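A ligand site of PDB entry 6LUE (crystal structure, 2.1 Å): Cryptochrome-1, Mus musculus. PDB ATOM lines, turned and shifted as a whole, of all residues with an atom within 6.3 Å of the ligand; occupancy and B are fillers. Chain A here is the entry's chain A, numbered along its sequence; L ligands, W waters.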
ATOM      1  N   GLY A 290     -33.547 -22.999   9.227  1.00  0.00           N
ATOM      2  CA  GLY A 290     -33.553 -22.389  10.552  1.00  0.00           C
ATOM      3  C   GLY A 290     -32.679 -21.152  10.661  1.00  0.00           C
ATOM      4  O   GLY A 290     -33.045 -20.195  11.351  1.00  0.00           O
ATOM      5  N   GLN A 291     -31.512 -21.157  10.013  1.00  0.00           N
ATOM      6  CA  GLN A 291     -30.658 -19.977  10.076  1.00  0.00           C
ATOM      7  C   GLN A 291     -31.368 -18.752   9.513  1.00  0.00           C
ATOM      8  O   GLN A 291     -31.345 -17.679  10.117  1.00  0.00           O
ATOM      9  CB  GLN A 291     -29.317 -20.215   9.356  1.00  0.00           C
ATOM     10  CG  GLN A 291     -28.369 -18.992   9.379  1.00  0.00           C
ATOM     11  CD  GLN A 291     -26.966 -19.298   8.861  1.00  0.00           C
ATOM     12  OE1 GLN A 291     -26.026 -18.522   9.085  1.00  0.00           O
ATOM     13  NE2 GLN A 291     -26.814 -20.404   8.157  1.00  0.00           N
ATOM     14  N   TRP A 294     -34.757 -17.851  11.742  1.00  0.00           N
ATOM     15  CA  TRP A 294     -34.482 -17.123  12.981  1.00  0.00           C
ATOM     16  C   TRP A 294     -34.185 -15.653  12.710  1.00  0.00           C
ATOM     17  O   TRP A 294     -34.577 -14.781  13.485  1.00  0.00           O
ATOM     18  CB  TRP A 294     -33.320 -17.782  13.731  1.00  0.00           C
ATOM     19  CG  TRP A 294     -33.750 -18.842  14.701  1.00  0.00           C
ATOM     20  CD1 TRP A 294     -33.595 -20.180  14.548  1.00  0.00           C
ATOM     21  CD2 TRP A 294     -34.394 -18.650  15.972  1.00  0.00           C
ATOM     22  NE1 TRP A 294     -34.101 -20.841  15.645  1.00  0.00           N
ATOM     23  CE2 TRP A 294     -34.593 -19.921  16.526  1.00  0.00           C
ATOM     24  CE3 TRP A 294     -34.821 -17.529  16.677  1.00  0.00           C
ATOM     25  CZ2 TRP A 294     -35.210 -20.109  17.769  1.00  0.00           C
ATOM     26  CZ3 TRP A 294     -35.421 -17.714  17.917  1.00  0.00           C
ATOM     27  CH2 TRP A 294     -35.611 -18.993  18.443  1.00  0.00           C
ATOM     28  N   ARG A 295     -33.504 -15.365  11.595  1.00  0.00           N
ATOM     29  CA  ARG A 295     -33.254 -13.969  11.229  1.00  0.00           C
ATOM     30  C   ARG A 295     -34.554 -13.247  10.894  1.00  0.00           C
ATOM     31  O   ARG A 295     -34.787 -12.117  11.341  1.00  0.00           O
ATOM     32  CB  ARG A 295     -32.283 -13.907  10.036  1.00  0.00           C
ATOM     33  CG  ARG A 295     -30.888 -14.455  10.334  1.00  0.00           C
ATOM     34  CD  ARG A 295     -30.050 -14.568   9.066  1.00  0.00           C
ATOM     35  NE  ARG A 295     -30.066 -13.324   8.284  1.00  0.00           N
ATOM     36  CZ  ARG A 295     -29.343 -12.247   8.558  1.00  0.00           C
ATOM     37  NH1 ARG A 295     -28.529 -12.241   9.614  1.00  0.00           N
ATOM     38  NH2 ARG A 295     -29.425 -11.159   7.781  1.00  0.00           N
ATOM     39  N   PHE A 298     -36.624 -12.136  14.204  1.00  0.00           N
ATOM     40  CA  PHE A 298     -36.239 -10.903  14.891  1.00  0.00           C
ATOM     41  C   PHE A 298     -36.545  -9.674  14.044  1.00  0.00           C
ATOM     42  O   PHE A 298     -36.984  -8.656  14.571  1.00  0.00           O
ATOM     43  CB  PHE A 298     -34.752 -10.966  15.273  1.00  0.00           C
ATOM     44  CG  PHE A 298     -34.471 -11.888  16.431  1.00  0.00           C
ATOM     45  CD1 PHE A 298     -35.077 -11.670  17.666  1.00  0.00           C
ATOM     46  CD2 PHE A 298     -33.654 -12.987  16.285  1.00  0.00           C
ATOM     47  CE1 PHE A 298     -34.830 -12.503  18.729  1.00  0.00           C
ATOM     48  CE2 PHE A 298     -33.409 -13.843  17.346  1.00  0.00           C
ATOM     49  CZ  PHE A 298     -34.008 -13.603  18.574  1.00  0.00           C
ATOM     50  N   HIS A 357     -22.066 -18.606  18.019  1.00  0.00           N
ATOM     51  CA  HIS A 357     -23.396 -18.462  18.607  1.00  0.00           C
ATOM     52  C   HIS A 357     -23.406 -18.741  20.113  1.00  0.00           C
ATOM     53  O   HIS A 357     -23.931 -17.951  20.895  1.00  0.00           O
ATOM     54  CB  HIS A 357     -24.364 -19.403  17.878  1.00  0.00           C
ATOM     55  CG  HIS A 357     -25.772 -19.364  18.410  1.00  0.00           C
ATOM     56  ND1 HIS A 357     -26.690 -18.411  18.013  1.00  0.00           N
ATOM     57  CD2 HIS A 357     -26.413 -20.153  19.296  1.00  0.00           C
ATOM     58  CE1 HIS A 357     -27.829 -18.618  18.637  1.00  0.00           C
ATOM     59  NE2 HIS A 357     -27.694 -19.667  19.420  1.00  0.00           N
ATOM     60  N   ARG A 360     -21.579 -16.181  22.143  1.00  0.00           N
ATOM     61  CA  ARG A 360     -22.384 -14.986  22.377  1.00  0.00           C
ATOM     62  C   ARG A 360     -23.285 -15.156  23.593  1.00  0.00           C
ATOM     63  O   ARG A 360     -23.435 -14.229  24.397  1.00  0.00           O
ATOM     64  CB  ARG A 360     -23.207 -14.648  21.132  1.00  0.00           C
ATOM     65  CG  ARG A 360     -22.366 -14.616  19.858  1.00  0.00           C
ATOM     66  CD  ARG A 360     -23.182 -14.291  18.605  1.00  0.00           C
ATOM     67  NE  ARG A 360     -22.429 -14.617  17.400  1.00  0.00           N
ATOM     68  CZ  ARG A 360     -22.774 -14.224  16.173  1.00  0.00           C
ATOM     69  NH1 ARG A 360     -23.871 -13.504  15.992  1.00  0.00           N
ATOM     70  NH2 ARG A 360     -22.028 -14.561  15.123  1.00  0.00           N
ATOM     71  N   HIS A 361     -23.883 -16.343  23.757  1.00  0.00           N
ATOM     72  CA  HIS A 361     -24.618 -16.640  24.991  1.00  0.00           C
ATOM     73  C   HIS A 361     -23.749 -16.400  26.229  1.00  0.00           C
ATOM     74  O   HIS A 361     -24.146 -15.712  27.167  1.00  0.00           O
ATOM     75  CB  HIS A 361     -25.126 -18.089  24.992  1.00  0.00           C
ATOM     76  CG  HIS A 361     -26.266 -18.342  24.051  1.00  0.00           C
ATOM     77  ND1 HIS A 361     -26.371 -17.740  22.820  1.00  0.00           N
ATOM     78  CD2 HIS A 361     -27.351 -19.147  24.169  1.00  0.00           C
ATOM     79  CE1 HIS A 361     -27.467 -18.154  22.216  1.00  0.00           C
ATOM     80  NE2 HIS A 361     -28.086 -19.009  23.011  1.00  0.00           N
ATOM     81  N   ALA A 364     -22.920 -12.636  26.884  1.00  0.00           N
ATOM     82  CA  ALA A 364     -24.131 -11.866  27.153  1.00  0.00           C
ATOM     83  C   ALA A 364     -24.669 -12.150  28.548  1.00  0.00           C
ATOM     84  O   ALA A 364     -25.101 -11.233  29.258  1.00  0.00           O
ATOM     85  CB  ALA A 364     -25.202 -12.158  26.101  1.00  0.00           C
ATOM     86  N   PHE A 383     -21.701  -4.879  20.749  1.00  0.00           N
ATOM     87  CA  PHE A 383     -21.811  -5.771  19.605  1.00  0.00           C
ATOM     88  C   PHE A 383     -22.088  -5.002  18.320  1.00  0.00           C
ATOM     89  O   PHE A 383     -21.649  -5.391  17.241  1.00  0.00           O
ATOM     90  CB  PHE A 383     -22.918  -6.803  19.830  1.00  0.00           C
ATOM     91  CG  PHE A 383     -22.493  -8.005  20.639  1.00  0.00           C
ATOM     92  CD1 PHE A 383     -21.379  -7.944  21.482  1.00  0.00           C
ATOM     93  CD2 PHE A 383     -23.223  -9.175  20.586  1.00  0.00           C
ATOM     94  CE1 PHE A 383     -21.000  -9.037  22.224  1.00  0.00           C
ATOM     95  CE2 PHE A 383     -22.845 -10.282  21.338  1.00  0.00           C
ATOM     96  CZ  PHE A 383     -21.730 -10.216  22.159  1.00  0.00           C
ATOM     97  N   LEU A 387     -19.615  -6.614  15.994  1.00  0.00           N
ATOM     98  CA  LEU A 387     -20.113  -7.893  15.461  1.00  0.00           C
ATOM     99  C   LEU A 387     -20.559  -7.731  14.016  1.00  0.00           C
ATOM    100  O   LEU A 387     -21.536  -7.024  13.740  1.00  0.00           O
ATOM    101  CB  LEU A 387     -21.279  -8.421  16.301  1.00  0.00           C
ATOM    102  CG  LEU A 387     -21.152  -9.739  17.074  1.00  0.00           C
ATOM    103  CD1 LEU A 387     -22.525 -10.165  17.569  1.00  0.00           C
ATOM    104  CD2 LEU A 387     -20.519 -10.824  16.229  1.00  0.00           C
ATOM    105  N   ASP A 389     -22.075  -9.778  11.892  1.00  0.00           N
ATOM    106  CA  ASP A 389     -23.356 -10.322  11.458  1.00  0.00           C
ATOM    107  C   ASP A 389     -24.527  -9.841  12.309  1.00  0.00           C
ATOM    108  O   ASP A 389     -25.599 -10.440  12.257  1.00  0.00           O
ATOM    109  CB  ASP A 389     -23.299 -11.858  11.418  1.00  0.00           C
ATOM    110  CG  ASP A 389     -23.080 -12.492  12.800  1.00  0.00           C
ATOM    111  OD1 ASP A 389     -23.032 -11.787  13.816  1.00  0.00           O
ATOM    112  OD2 ASP A 389     -22.944 -13.732  12.854  1.00  0.00           O
ATOM    113  N   ALA A 390     -24.356  -8.758  13.060  1.00  0.00           N
ATOM    114  CA  ALA A 390     -25.351  -8.356  14.058  1.00  0.00           C
ATOM    115  C   ALA A 390     -26.194  -7.212  13.501  1.00  0.00           C
ATOM    116  O   ALA A 390     -25.952  -6.042  13.794  1.00  0.00           O
ATOM    117  CB  ALA A 390     -24.684  -7.962  15.362  1.00  0.00           C
ATOM    118  N   ASP A 391     -27.197  -7.566  12.699  1.00  0.00           N
ATOM    119  CA  ASP A 391     -28.193  -6.593  12.271  1.00  0.00           C
ATOM    120  C   ASP A 391     -28.833  -5.929  13.488  1.00  0.00           C
ATOM    121  O   ASP A 391     -28.927  -6.522  14.568  1.00  0.00           O
ATOM    122  CB  ASP A 391     -29.291  -7.278  11.433  1.00  0.00           C
ATOM    123  CG  ASP A 391     -28.733  -8.348  10.493  1.00  0.00           C
ATOM    124  OD1 ASP A 391     -28.271  -9.401  10.974  1.00  0.00           O
ATOM    125  OD2 ASP A 391     -28.776  -8.130   9.263  1.00  0.00           O
ATOM    126  N   ILE A 394     -31.668  -8.036  14.898  1.00  0.00           N
ATOM    127  CA  ILE A 394     -31.226  -9.262  15.534  1.00  0.00           C
ATOM    128  C   ILE A 394     -30.440  -8.963  16.809  1.00  0.00           C
ATOM    129  O   ILE A 394     -30.632  -9.606  17.847  1.00  0.00           O
ATOM    130  CB  ILE A 394     -30.402 -10.107  14.537  1.00  0.00           C
ATOM    131  CG1 ILE A 394     -31.292 -10.547  13.362  1.00  0.00           C
ATOM    132  CG2 ILE A 394     -29.809 -11.324  15.208  1.00  0.00           C
ATOM    133  CD1 ILE A 394     -30.535 -11.310  12.273  1.00  0.00           C
ATOM    134  N   ASN A 395     -29.557  -7.967  16.758  1.00  0.00           N
ATOM    135  CA  ASN A 395     -28.798  -7.558  17.931  1.00  0.00           C
ATOM    136  C   ASN A 395     -29.720  -7.181  19.092  1.00  0.00           C
ATOM    137  O   ASN A 395     -29.589  -7.723  20.203  1.00  0.00           O
ATOM    138  CB  ASN A 395     -27.876  -6.384  17.565  1.00  0.00           C
ATOM    139  CG  ASN A 395     -26.711  -6.226  18.529  1.00  0.00           C
ATOM    140  OD1 ASN A 395     -26.395  -7.117  19.321  1.00  0.00           O
ATOM    141  ND2 ASN A 395     -26.049  -5.078  18.444  1.00  0.00           N
ATOM    142  N   ALA A 396     -30.656  -6.261  18.865  1.00  0.00           N
ATOM    143  CA  ALA A 396     -31.556  -5.843  19.938  1.00  0.00           C
ATOM    144  C   ALA A 396     -32.410  -7.011  20.419  1.00  0.00           C
ATOM    145  O   ALA A 396     -32.517  -7.257  21.636  1.00  0.00           O
ATOM    146  CB  ALA A 396     -32.440  -4.685  19.484  1.00  0.00           C
ATOM    147  N   GLY A 397     -33.034  -7.736  19.492  1.00  0.00           N
ATOM    148  CA  GLY A 397     -33.846  -8.882  19.871  1.00  0.00           C
ATOM    149  C   GLY A 397     -33.064  -9.920  20.648  1.00  0.00           C
ATOM    150  O   GLY A 397     -33.565 -10.503  21.613  1.00  0.00           O
ATOM    151  N   SER A 398     -31.810 -10.173  20.232  1.00  0.00           N
ATOM    152  CA  SER A 398     -31.001 -11.177  20.899  1.00  0.00           C
ATOM    153  C   SER A 398     -30.664 -10.763  22.323  1.00  0.00           C
ATOM    154  O   SER A 398     -30.808 -11.556  23.259  1.00  0.00           O
ATOM    155  CB  SER A 398     -29.719 -11.439  20.102  1.00  0.00           C
ATOM    156  OG  SER A 398     -29.998 -12.252  18.982  1.00  0.00           O
ATOM    157  N   TRP A 399     -30.240  -9.495  22.510  1.00  0.00           N
ATOM    158  CA  TRP A 399     -29.854  -9.057  23.848  1.00  0.00           C
ATOM    159  C   TRP A 399     -31.044  -9.041  24.790  1.00  0.00           C
ATOM    160  O   TRP A 399     -30.870  -9.287  25.987  1.00  0.00           O
ATOM    161  CB  TRP A 399     -29.196  -7.671  23.777  1.00  0.00           C
ATOM    162  CG  TRP A 399     -27.714  -7.750  23.488  1.00  0.00           C
ATOM    163  CD1 TRP A 399     -27.123  -7.549  22.289  1.00  0.00           C
ATOM    164  CD2 TRP A 399     -26.673  -8.094  24.407  1.00  0.00           C
ATOM    165  NE1 TRP A 399     -25.768  -7.745  22.393  1.00  0.00           N
ATOM    166  CE2 TRP A 399     -25.466  -8.083  23.678  1.00  0.00           C
ATOM    167  CE3 TRP A 399     -26.636  -8.411  25.767  1.00  0.00           C
ATOM    168  CZ2 TRP A 399     -24.235  -8.372  24.281  1.00  0.00           C
ATOM    169  CZ3 TRP A 399     -25.413  -8.703  26.354  1.00  0.00           C
ATOM    170  CH2 TRP A 399     -24.228  -8.675  25.614  1.00  0.00           C
ATOM    171  N   TRP A 401     -33.565 -11.242  24.451  1.00  0.00           N
ATOM    172  CA  TRP A 401     -33.774 -12.674  24.634  1.00  0.00           C
ATOM    173  C   TRP A 401     -32.852 -13.230  25.711  1.00  0.00           C
ATOM    174  O   TRP A 401     -33.303 -13.884  26.657  1.00  0.00           O
ATOM    175  CB  TRP A 401     -33.551 -13.381  23.297  1.00  0.00           C
ATOM    176  CG  TRP A 401     -33.793 -14.856  23.269  1.00  0.00           C
ATOM    177  CD1 TRP A 401     -33.072 -15.821  23.902  1.00  0.00           C
ATOM    178  CD2 TRP A 401     -34.840 -15.536  22.549  1.00  0.00           C
ATOM    179  NE1 TRP A 401     -33.606 -17.058  23.633  1.00  0.00           N
ATOM    180  CE2 TRP A 401     -34.687 -16.916  22.813  1.00  0.00           C
ATOM    181  CE3 TRP A 401     -35.875 -15.127  21.714  1.00  0.00           C
ATOM    182  CZ2 TRP A 401     -35.532 -17.878  22.261  1.00  0.00           C
ATOM    183  CZ3 TRP A 401     -36.732 -16.076  21.179  1.00  0.00           C
ATOM    184  CH2 TRP A 401     -36.552 -17.436  21.446  1.00  0.00           C
ATOM    185  N   LEU A 402     -31.542 -12.967  25.599  1.00  0.00           N
ATOM    186  CA  LEU A 402     -30.560 -13.569  26.492  1.00  0.00           C
ATOM    187  C   LEU A 402     -30.457 -12.878  27.854  1.00  0.00           C
ATOM    188  O   LEU A 402     -29.852 -13.440  28.775  1.00  0.00           O
ATOM    189  CB  LEU A 402     -29.189 -13.574  25.816  1.00  0.00           C
ATOM    190  CG  LEU A 402     -29.069 -14.488  24.589  1.00  0.00           C
ATOM    191  CD1 LEU A 402     -27.902 -14.047  23.725  1.00  0.00           C
ATOM    192  CD2 LEU A 402     -28.898 -15.945  25.019  1.00  0.00           C
HETATM  193  C1  LIG L   1     -28.665 -14.757  16.698  1.00  0.00           C
HETATM  194  C2  LIG L   1     -28.675 -15.509  14.488  1.00  0.00           C
HETATM  195  C3  LIG L   1     -26.904 -13.433  17.892  1.00  0.00           C
HETATM  196  C4  LIG L   1     -26.637 -12.445  18.975  1.00  0.00           C
HETATM  197  C5  LIG L   1     -26.592 -12.884  20.326  1.00  0.00           C
HETATM  198  C6  LIG L   1     -26.373 -11.986  21.370  1.00  0.00           C
HETATM  199  C7  LIG L   1     -26.220 -10.621  21.121  1.00  0.00           C
HETATM  200  C8  LIG L   1     -26.293 -10.191  19.812  1.00  0.00           C
HETATM  201  C9  LIG L   1     -26.497 -11.112  18.810  1.00  0.00           C
HETATM  202  C10 LIG L   1     -30.029 -16.564  15.975  1.00  0.00           C
HETATM  203  C11 LIG L   1     -29.603 -15.721  17.037  1.00  0.00           C
HETATM  204  C12 LIG L   1     -30.301 -16.097  18.265  1.00  0.00           C
HETATM  205  C13 LIG L   1     -31.150 -17.107  18.152  1.00  0.00           C
HETATM  206  C14 LIG L   1     -31.955 -17.679  19.251  1.00  0.00           C
HETATM  207  C15 LIG L   1     -31.475 -17.184  20.617  1.00  0.00           C
HETATM  208  C16 LIG L   1     -31.078 -15.725  20.637  1.00  0.00           C
HETATM  209  C17 LIG L   1     -30.059 -15.379  19.555  1.00  0.00           C
HETATM  210  N1  LIG L   1     -28.197 -13.840  17.682  1.00  0.00           N
HETATM  211  N2  LIG L   1     -28.191 -14.621  15.424  1.00  0.00           N
HETATM  212  N3  LIG L   1     -29.582 -16.483  14.696  1.00  0.00           N
HETATM  213  O1  LIG L   1     -26.023 -13.842  17.184  1.00  0.00           O
HETATM  214  S1  LIG L   1     -31.173 -17.708  16.528  1.00  0.00           S
HETATM  215 BR1  LIG L   1     -26.557 -10.348  17.017  1.00  0.00          BR
HETATM  216  O   HOH W   1     -26.346 -13.054  13.678  1.00  0.00           O
HETATM  217  O   HOH W   2     -25.614 -16.425  16.060  1.00  0.00           O
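A nitrogen (N1) of the ligand lies within hydrogen-bond range of the side-chain hydroxyl (OG) of Ser 398 (2.7 Å). An oxygen (O1) of the ligand sits at hydrogen-bond distance from the guanidinium group (NH1) of Arg 360, at 2.5 Å.
OG of Ser 398 sits at hydrogen-bond distance from O of Ile 394, at 2.9 Å. O of His 357 lies within hydrogen-bond range of ND1 of His 361, 3.1 Å away. NH2 of Arg 360 lies within salt-bridge range of OD2 of Asp 389, 2.6 Å away. NE1 of Trp 399 lies close to OD1 of Asn 395, 3.2 Å away.
Trp 294 touches the ligand. CE2 of Phe 298 touches C12 of the ligand, 3.9 Å away. His 357 touches the ligand. Phe 383 touches the ligand (CD2 to C8, 3.3 Å). Ala 390 touches the ligand. CG2 of Ile 394 touches N2 of the ligand, at 3.7 Å. OD1 of Asn 395 touches C8 of the ligand (3.1 Å). Trp 399 touches the ligand (NE1 to C7, 3.2 Å). Trp 401 touches the ligand (NE1 to C15, 3.7 Å). CD1 of Leu 402 touches C6 of the ligand (3.5 Å). Hydrophobic or aromatic side chains that line the ligand: Trp 294, Phe 298, His 357, Phe 383, Ala 390, Ile 394, Trp 399, Trp 401 and Leu 402. Of the 22 residues printed, 12 come within 4 Å of the ligand.
Water W2 lies within hydrogen-bond range of O1 of the ligand (2.8 Å), ND1 of His 357 (3.0 Å) and NH1 of Arg 360 (3.4 Å). Water W1 lies within hydrogen-bond range of N2 of the ligand (3.0 Å), O of Asp 389 (3.1 Å) and NH1 of Arg 360 (3.4 Å).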
